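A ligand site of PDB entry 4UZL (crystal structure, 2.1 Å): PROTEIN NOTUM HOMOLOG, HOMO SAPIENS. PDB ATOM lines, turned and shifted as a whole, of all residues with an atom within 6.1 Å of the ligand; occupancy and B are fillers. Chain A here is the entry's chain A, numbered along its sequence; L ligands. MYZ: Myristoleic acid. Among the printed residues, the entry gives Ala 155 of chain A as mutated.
N of Trp 51 lies within hydrogen-bond range of O2 of the ligand (2.8 Å). An oxygen (O2) of the ligand is in hydrogen-bond range of the backbone NH (N) of Ala 156. A ring nitrogen (NE2) of His 312 lies within hydrogen-bond range of an oxygen (O1) of the ligand. An oxygen (O2) of the ligand is in hydrogen-bond range of the backbone NH (N) of Gly 50.
OH of Tyr 105 lies within hydrogen-bond range of O of Trp 51, 2.5 Å away. OG1 of Thr 159 is in hydrogen-bond range of O of Gly 189 (2.8 Å). The backbone NH (N) of Glu 313 lies within hydrogen-bond range of the side-chain hydroxyl (OG) of Ser 188 (2.7 Å). The backbone NH (N) of Val 110 sits at hydrogen-bond distance from the side-chain hydroxyl (OH) of Tyr 105, 3.0 Å away.
Residues that only touch the ligand: Tyr 52 (3.7 Å), Val 110 (3.9 Å), Ala 155 (3.1 Å), Thr 159 (3.5 Å), Phe 191 (3.7 Å), Pro 210 (3.9 Å), Ile 214 (3.4 Å), Ala 265 (3.8 Å), Val 269 (3.8 Å) and Glu 313 (3.9 Å). Within 4 Å of the ligand: Gly 50, Trp 51, Tyr 52, Val 110, Ala 155, Ala 156, Thr 159, Phe 191, Pro 210, Ile 214, Ala 265, Val 269, His 312 and Glu 313. Along chain A the residues within 4 Å of the ligand span positions 50 to 313. The nearest printed residue that does not touch the ligand is Phe 242 (4.01 Å).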
ATOM      1  N   GLY A  49     -20.347   9.874  27.691  1.00  0.00           N
ATOM      2  CA  GLY A  49     -18.989   9.360  27.763  1.00  0.00           C
ATOM      3  C   GLY A  49     -18.602   8.950  29.185  1.00  0.00           C
ATOM      4  O   GLY A  49     -19.420   8.964  30.111  1.00  0.00           O
ATOM      5  N   GLY A  50     -17.357   8.515  29.338  1.00  0.00           N
ATOM      6  CA  GLY A  50     -16.811   8.177  30.661  1.00  0.00           C
ATOM      7  C   GLY A  50     -15.811   7.048  30.636  1.00  0.00           C
ATOM      8  O   GLY A  50     -15.955   6.033  31.366  1.00  0.00           O
ATOM      9  N   TRP A  51     -14.792   7.218  29.815  1.00  0.00           N
ATOM     10  CA  TRP A  51     -13.745   6.220  29.634  1.00  0.00           C
ATOM     11  C   TRP A  51     -14.287   4.850  29.204  1.00  0.00           C
ATOM     12  O   TRP A  51     -15.120   4.771  28.298  1.00  0.00           O
ATOM     13  CB  TRP A  51     -12.864   6.125  30.914  1.00  0.00           C
ATOM     14  CG  TRP A  51     -12.057   7.360  31.118  1.00  0.00           C
ATOM     15  CD1 TRP A  51     -12.361   8.435  31.899  1.00  0.00           C
ATOM     16  CD2 TRP A  51     -10.832   7.689  30.449  1.00  0.00           C
ATOM     17  NE1 TRP A  51     -11.392   9.395  31.783  1.00  0.00           N
ATOM     18  CE2 TRP A  51     -10.437   8.954  30.905  1.00  0.00           C
ATOM     19  CE3 TRP A  51     -10.016   7.008  29.544  1.00  0.00           C
ATOM     20  CZ2 TRP A  51      -9.270   9.556  30.493  1.00  0.00           C
ATOM     21  CZ3 TRP A  51      -8.864   7.594  29.144  1.00  0.00           C
ATOM     22  CH2 TRP A  51      -8.498   8.860  29.616  1.00  0.00           C
ATOM     23  N   TYR A  52     -13.808   3.793  29.846  1.00  0.00           N
ATOM     24  CA  TYR A  52     -13.962   2.398  29.441  1.00  0.00           C
ATOM     25  C   TYR A  52     -13.115   1.499  30.395  1.00  0.00           C
ATOM     26  O   TYR A  52     -12.281   1.998  31.153  1.00  0.00           O
ATOM     27  CB  TYR A  52     -13.457   2.174  28.013  1.00  0.00           C
ATOM     28  CG  TYR A  52     -12.082   2.763  27.683  1.00  0.00           C
ATOM     29  CD1 TYR A  52     -10.901   2.130  28.083  1.00  0.00           C
ATOM     30  CD2 TYR A  52     -11.977   3.927  26.930  1.00  0.00           C
ATOM     31  CE1 TYR A  52      -9.669   2.660  27.790  1.00  0.00           C
ATOM     32  CE2 TYR A  52     -10.743   4.471  26.607  1.00  0.00           C
ATOM     33  CZ  TYR A  52      -9.585   3.836  27.034  1.00  0.00           C
ATOM     34  OH  TYR A  52      -8.350   4.372  26.700  1.00  0.00           O
ATOM     35  N   TYR A 105     -24.204   5.923  29.689  1.00  0.00           N
ATOM     36  CA  TYR A 105     -23.135   4.996  29.342  1.00  0.00           C
ATOM     37  C   TYR A 105     -22.878   3.995  30.494  1.00  0.00           C
ATOM     38  O   TYR A 105     -22.250   4.333  31.494  1.00  0.00           O
ATOM     39  CB  TYR A 105     -21.879   5.821  29.095  1.00  0.00           C
ATOM     40  CG  TYR A 105     -20.622   5.135  28.668  1.00  0.00           C
ATOM     41  CD1 TYR A 105     -20.637   4.115  27.742  1.00  0.00           C
ATOM     42  CD2 TYR A 105     -19.408   5.572  29.133  1.00  0.00           C
ATOM     43  CE1 TYR A 105     -19.462   3.522  27.333  1.00  0.00           C
ATOM     44  CE2 TYR A 105     -18.240   4.976  28.735  1.00  0.00           C
ATOM     45  CZ  TYR A 105     -18.257   3.974  27.831  1.00  0.00           C
ATOM     46  OH  TYR A 105     -17.055   3.399  27.429  1.00  0.00           O
ATOM     47  N   VAL A 110     -16.971   1.940  24.851  1.00  0.00           N
ATOM     48  CA  VAL A 110     -17.052   2.978  23.828  1.00  0.00           C
ATOM     49  C   VAL A 110     -18.184   2.656  22.839  1.00  0.00           C
ATOM     50  O   VAL A 110     -18.068   2.898  21.630  1.00  0.00           O
ATOM     51  CB  VAL A 110     -15.700   3.172  23.106  1.00  0.00           C
ATOM     52  CG1 VAL A 110     -15.675   4.475  22.316  1.00  0.00           C
ATOM     53  CG2 VAL A 110     -14.551   3.164  24.100  1.00  0.00           C
ATOM     54  N   SER A 154     -20.442  12.948  23.620  1.00  0.00           N
ATOM     55  CA  SER A 154     -19.182  13.506  24.091  1.00  0.00           C
ATOM     56  C   SER A 154     -18.245  12.439  24.650  1.00  0.00           C
ATOM     57  O   SER A 154     -18.674  11.514  25.375  1.00  0.00           O
ATOM     58  CB  SER A 154     -19.417  14.514  25.189  1.00  0.00           C
ATOM     59  OG  SER A 154     -20.263  15.568  24.775  1.00  0.00           O
ATOM     60  N   ALA A 155     -16.970  12.608  24.325  1.00  0.00           N
ATOM     61  CA  ALA A 155     -15.881  11.771  24.819  1.00  0.00           C
ATOM     62  C   ALA A 155     -16.034  10.356  24.294  1.00  0.00           C
ATOM     63  O   ALA A 155     -16.145  10.198  23.080  1.00  0.00           O
ATOM     64  CB  ALA A 155     -15.798  11.801  26.352  1.00  0.00           C
ATOM     65  N   ALA A 156     -16.078   9.340  25.151  1.00  0.00           N
ATOM     66  CA  ALA A 156     -16.349   7.989  24.656  1.00  0.00           C
ATOM     67  C   ALA A 156     -17.632   7.947  23.819  1.00  0.00           C
ATOM     68  O   ALA A 156     -17.733   7.181  22.872  1.00  0.00           O
ATOM     69  CB  ALA A 156     -16.425   7.000  25.817  1.00  0.00           C
ATOM     70  N   GLY A 157     -18.622   8.760  24.201  1.00  0.00           N
ATOM     71  CA  GLY A 157     -19.838   8.894  23.455  1.00  0.00           C
ATOM     72  C   GLY A 157     -19.633   9.573  22.073  1.00  0.00           C
ATOM     73  O   GLY A 157     -20.321   9.253  21.126  1.00  0.00           O
ATOM     74  N   THR A 159     -16.761   9.184  20.341  1.00  0.00           N
ATOM     75  CA  THR A 159     -16.286   8.058  19.578  1.00  0.00           C
ATOM     76  C   THR A 159     -17.399   7.056  19.260  1.00  0.00           C
ATOM     77  O   THR A 159     -17.356   6.435  18.207  1.00  0.00           O
ATOM     78  CB  THR A 159     -15.120   7.371  20.276  1.00  0.00           C
ATOM     79  OG1 THR A 159     -14.135   8.353  20.599  1.00  0.00           O
ATOM     80  CG2 THR A 159     -14.520   6.317  19.382  1.00  0.00           C
ATOM     81  N   SER A 188     -15.392  15.787  21.317  1.00  0.00           N
ATOM     82  CA  SER A 188     -14.264  15.276  22.088  1.00  0.00           C
ATOM     83  C   SER A 188     -14.074  13.768  21.931  1.00  0.00           C
ATOM     84  O   SER A 188     -13.759  13.076  22.893  1.00  0.00           O
ATOM     85  CB  SER A 188     -14.421  15.635  23.545  1.00  0.00           C
ATOM     86  OG  SER A 188     -14.429  17.034  23.668  1.00  0.00           O
ATOM     87  N   GLY A 189     -14.288  13.272  20.711  1.00  0.00           N
ATOM     88  CA  GLY A 189     -14.226  11.846  20.413  1.00  0.00           C
ATOM     89  C   GLY A 189     -13.232  11.488  19.306  1.00  0.00           C
ATOM     90  O   GLY A 189     -13.240  10.374  18.804  1.00  0.00           O
ATOM     91  N   PHE A 191      -9.535  11.113  18.287  1.00  0.00           N
ATOM     92  CA  PHE A 191      -8.232  10.943  18.896  1.00  0.00           C
ATOM     93  C   PHE A 191      -7.230  10.305  17.935  1.00  0.00           C
ATOM     94  O   PHE A 191      -7.608   9.609  16.973  1.00  0.00           O
ATOM     95  CB  PHE A 191      -8.355  10.096  20.166  1.00  0.00           C
ATOM     96  CG  PHE A 191      -9.254  10.705  21.205  1.00  0.00           C
ATOM     97  CD1 PHE A 191      -8.821  11.769  22.001  1.00  0.00           C
ATOM     98  CD2 PHE A 191     -10.554  10.208  21.411  1.00  0.00           C
ATOM     99  CE1 PHE A 191      -9.650  12.329  22.948  1.00  0.00           C
ATOM    100  CE2 PHE A 191     -11.383  10.777  22.369  1.00  0.00           C
ATOM    101  CZ  PHE A 191     -10.935  11.831  23.137  1.00  0.00           C
ATOM    102  N   LEU A 192      -5.958  10.529  18.249  1.00  0.00           N
ATOM    103  CA  LEU A 192      -4.849  10.000  17.473  1.00  0.00           C
ATOM    104  C   LEU A 192      -4.250   8.733  18.111  1.00  0.00           C
ATOM    105  O   LEU A 192      -4.083   8.660  19.343  1.00  0.00           O
ATOM    106  CB  LEU A 192      -3.771  11.086  17.354  1.00  0.00           C
ATOM    107  CG  LEU A 192      -4.294  12.428  16.825  1.00  0.00           C
ATOM    108  CD1 LEU A 192      -3.335  13.569  17.154  1.00  0.00           C
ATOM    109  CD2 LEU A 192      -4.555  12.342  15.332  1.00  0.00           C
ATOM    110  N   PRO A 210      -2.964   4.744  23.679  1.00  0.00           N
ATOM    111  CA  PRO A 210      -4.209   4.723  22.901  1.00  0.00           C
ATOM    112  C   PRO A 210      -4.347   3.505  21.999  1.00  0.00           C
ATOM    113  O   PRO A 210      -5.442   2.975  21.865  1.00  0.00           O
ATOM    114  CB  PRO A 210      -4.124   6.008  22.057  1.00  0.00           C
ATOM    115  CG  PRO A 210      -2.683   6.387  22.058  1.00  0.00           C
ATOM    116  CD  PRO A 210      -2.179   5.967  23.407  1.00  0.00           C
ATOM    117  N   THR A 211      -3.250   3.084  21.371  1.00  0.00           N
ATOM    118  CA  THR A 211      -3.268   1.961  20.429  1.00  0.00           C
ATOM    119  C   THR A 211      -3.471   0.614  21.131  1.00  0.00           C
ATOM    120  O   THR A 211      -4.256  -0.215  20.682  1.00  0.00           O
ATOM    121  CB  THR A 211      -1.972   1.931  19.573  1.00  0.00           C
ATOM    122  OG1 THR A 211      -1.909   3.133  18.786  1.00  0.00           O
ATOM    123  CG2 THR A 211      -1.953   0.715  18.645  1.00  0.00           C
ATOM    124  N   ALA A 213      -4.624   0.082  24.298  1.00  0.00           N
ATOM    125  CA  ALA A 213      -5.924   0.124  24.979  1.00  0.00           C
ATOM    126  C   ALA A 213      -7.072  -0.544  24.214  1.00  0.00           C
ATOM    127  O   ALA A 213      -7.815  -1.354  24.774  1.00  0.00           O
ATOM    128  CB  ALA A 213      -6.285   1.568  25.293  1.00  0.00           C
ATOM    129  N   ILE A 214      -7.188  -0.212  22.922  1.00  0.00           N
ATOM    130  CA  ILE A 214      -8.295  -0.655  22.070  1.00  0.00           C
ATOM    131  C   ILE A 214      -8.133  -2.066  21.475  1.00  0.00           C
ATOM    132  O   ILE A 214      -9.146  -2.749  21.218  1.00  0.00           O
ATOM    133  CB  ILE A 214      -8.544   0.332  20.901  1.00  0.00           C
ATOM    134  CG1 ILE A 214      -8.653   1.791  21.397  1.00  0.00           C
ATOM    135  CG2 ILE A 214      -9.822  -0.032  20.144  1.00  0.00           C
ATOM    136  CD1 ILE A 214      -9.752   2.042  22.418  1.00  0.00           C
ATOM    137  N   PHE A 242     -11.485   2.650  15.561  1.00  0.00           N
ATOM    138  CA  PHE A 242     -11.790   3.521  16.727  1.00  0.00           C
ATOM    139  C   PHE A 242     -11.210   4.941  16.598  1.00  0.00           C
ATOM    140  O   PHE A 242     -11.559   5.863  17.364  1.00  0.00           O
ATOM    141  CB  PHE A 242     -11.277   2.895  18.043  1.00  0.00           C
ATOM    142  CG  PHE A 242     -12.183   1.835  18.610  1.00  0.00           C
ATOM    143  CD1 PHE A 242     -12.342   0.622  17.967  1.00  0.00           C
ATOM    144  CD2 PHE A 242     -12.872   2.062  19.784  1.00  0.00           C
ATOM    145  CE1 PHE A 242     -13.184  -0.354  18.480  1.00  0.00           C
ATOM    146  CE2 PHE A 242     -13.714   1.096  20.308  1.00  0.00           C
ATOM    147  CZ  PHE A 242     -13.880  -0.107  19.646  1.00  0.00           C
ATOM    148  N   PHE A 243     -10.318   5.118  15.624  1.00  0.00           N
ATOM    149  CA  PHE A 243      -9.647   6.405  15.446  1.00  0.00           C
ATOM    150  C   PHE A 243     -10.268   7.225  14.302  1.00  0.00           C
ATOM    151  O   PHE A 243     -10.253   6.808  13.136  1.00  0.00           O
ATOM    152  CB  PHE A 243      -8.143   6.166  15.288  1.00  0.00           C
ATOM    153  CG  PHE A 243      -7.532   5.547  16.488  1.00  0.00           C
ATOM    154  CD1 PHE A 243      -7.561   4.153  16.658  1.00  0.00           C
ATOM    155  CD2 PHE A 243      -7.003   6.333  17.499  1.00  0.00           C
ATOM    156  CE1 PHE A 243      -7.048   3.585  17.809  1.00  0.00           C
ATOM    157  CE2 PHE A 243      -6.497   5.768  18.638  1.00  0.00           C
ATOM    158  CZ  PHE A 243      -6.512   4.390  18.796  1.00  0.00           C
ATOM    159  N   ALA A 265      -8.096  14.419  27.811  1.00  0.00           N
ATOM    160  CA  ALA A 265      -8.087  12.960  27.837  1.00  0.00           C
ATOM    161  C   ALA A 265      -6.959  12.434  26.969  1.00  0.00           C
ATOM    162  O   ALA A 265      -6.199  11.572  27.411  1.00  0.00           O
ATOM    163  CB  ALA A 265      -9.418  12.393  27.367  1.00  0.00           C
ATOM    164  N   GLN A 266      -6.851  12.953  25.753  1.00  0.00           N
ATOM    165  CA  GLN A 266      -5.715  12.655  24.865  1.00  0.00           C
ATOM    166  C   GLN A 266      -4.385  12.750  25.608  1.00  0.00           C
ATOM    167  O   GLN A 266      -3.543  11.857  25.506  1.00  0.00           O
ATOM    168  CB  GLN A 266      -5.699  13.620  23.673  1.00  0.00           C
ATOM    169  CG  GLN A 266      -4.560  13.413  22.674  1.00  0.00           C
ATOM    170  CD  GLN A 266      -4.837  12.322  21.657  1.00  0.00           C
ATOM    171  OE1 GLN A 266      -5.767  12.436  20.860  1.00  0.00           O
ATOM    172  NE2 GLN A 266      -3.996  11.288  21.634  1.00  0.00           N
ATOM    173  N   VAL A 269      -3.617   9.952  28.396  1.00  0.00           N
ATOM    174  CA  VAL A 269      -3.149   8.667  27.835  1.00  0.00           C
ATOM    175  C   VAL A 269      -1.833   8.782  27.046  1.00  0.00           C
ATOM    176  O   VAL A 269      -1.248   7.777  26.659  1.00  0.00           O
ATOM    177  CB  VAL A 269      -4.212   7.974  26.961  1.00  0.00           C
ATOM    178  CG1 VAL A 269      -5.409   7.572  27.810  1.00  0.00           C
ATOM    179  CG2 VAL A 269      -4.647   8.837  25.778  1.00  0.00           C
ATOM    180  N   HIS A 312     -12.114  19.464  27.660  1.00  0.00           N
ATOM    181  CA  HIS A 312     -12.614  18.139  27.335  1.00  0.00           C
ATOM    182  C   HIS A 312     -14.139  18.136  27.369  1.00  0.00           C
ATOM    183  O   HIS A 312     -14.738  18.383  28.425  1.00  0.00           O
ATOM    184  CB  HIS A 312     -12.052  17.138  28.349  1.00  0.00           C
ATOM    185  CG  HIS A 312     -12.394  15.705  28.051  1.00  0.00           C
ATOM    186  ND1 HIS A 312     -12.214  15.123  26.813  1.00  0.00           N
ATOM    187  CD2 HIS A 312     -12.890  14.730  28.857  1.00  0.00           C
ATOM    188  CE1 HIS A 312     -12.582  13.860  26.868  1.00  0.00           C
ATOM    189  NE2 HIS A 312     -12.996  13.587  28.096  1.00  0.00           N
ATOM    190  N   GLU A 313     -14.769  17.875  26.225  1.00  0.00           N
ATOM    191  CA  GLU A 313     -16.250  17.899  26.085  1.00  0.00           C
ATOM    192  C   GLU A 313     -16.819  19.308  26.099  1.00  0.00           C
ATOM    193  O   GLU A 313     -16.220  20.225  26.654  1.00  0.00           O
ATOM    194  CB  GLU A 313     -16.987  17.071  27.180  1.00  0.00           C
ATOM    195  CG  GLU A 313     -16.377  15.714  27.437  1.00  0.00           C
ATOM    196  CD  GLU A 313     -17.218  14.848  28.372  1.00  0.00           C
ATOM    197  OE1 GLU A 313     -17.873  15.370  29.291  1.00  0.00           O
ATOM    198  OE2 GLU A 313     -17.225  13.624  28.179  1.00  0.00           O
HETATM  199  C1  MYZ L   1     -13.996  10.164  28.365  1.00  0.00           C
HETATM  200  O1  MYZ L   1     -14.532  11.010  29.114  1.00  0.00           O
HETATM  201  O2  MYZ L   1     -14.630   9.233  27.810  1.00  0.00           O
HETATM  202  C2  MYZ L   1     -12.531  10.272  28.096  1.00  0.00           C
HETATM  203  C3  MYZ L   1     -12.073   9.081  27.284  1.00  0.00           C
HETATM  204  C4  MYZ L   1     -12.432   9.160  25.803  1.00  0.00           C
HETATM  205  C5  MYZ L   1     -12.637   7.727  25.334  1.00  0.00           C
HETATM  206  C6  MYZ L   1     -12.477   7.559  23.842  1.00  0.00           C
HETATM  207  C7  MYZ L   1     -12.082   6.128  23.529  1.00  0.00           C
HETATM  208  C8  MYZ L   1     -12.091   5.938  22.023  1.00  0.00           C
HETATM  209  C9  MYZ L   1     -10.934   5.080  21.572  1.00  0.00           C
HETATM  210  C10 MYZ L   1      -9.663   5.486  21.555  1.00  0.00           C
HETATM  211  C11 MYZ L   1      -9.177   6.870  21.969  1.00  0.00           C
HETATM  212  C12 MYZ L   1      -7.848   6.764  22.719  1.00  0.00           C
HETATM  213  C13 MYZ L   1      -7.965   7.222  24.172  1.00  0.00           C
HETATM  214  C14 MYZ L   1      -8.167   8.727  24.294  1.00  0.00           C
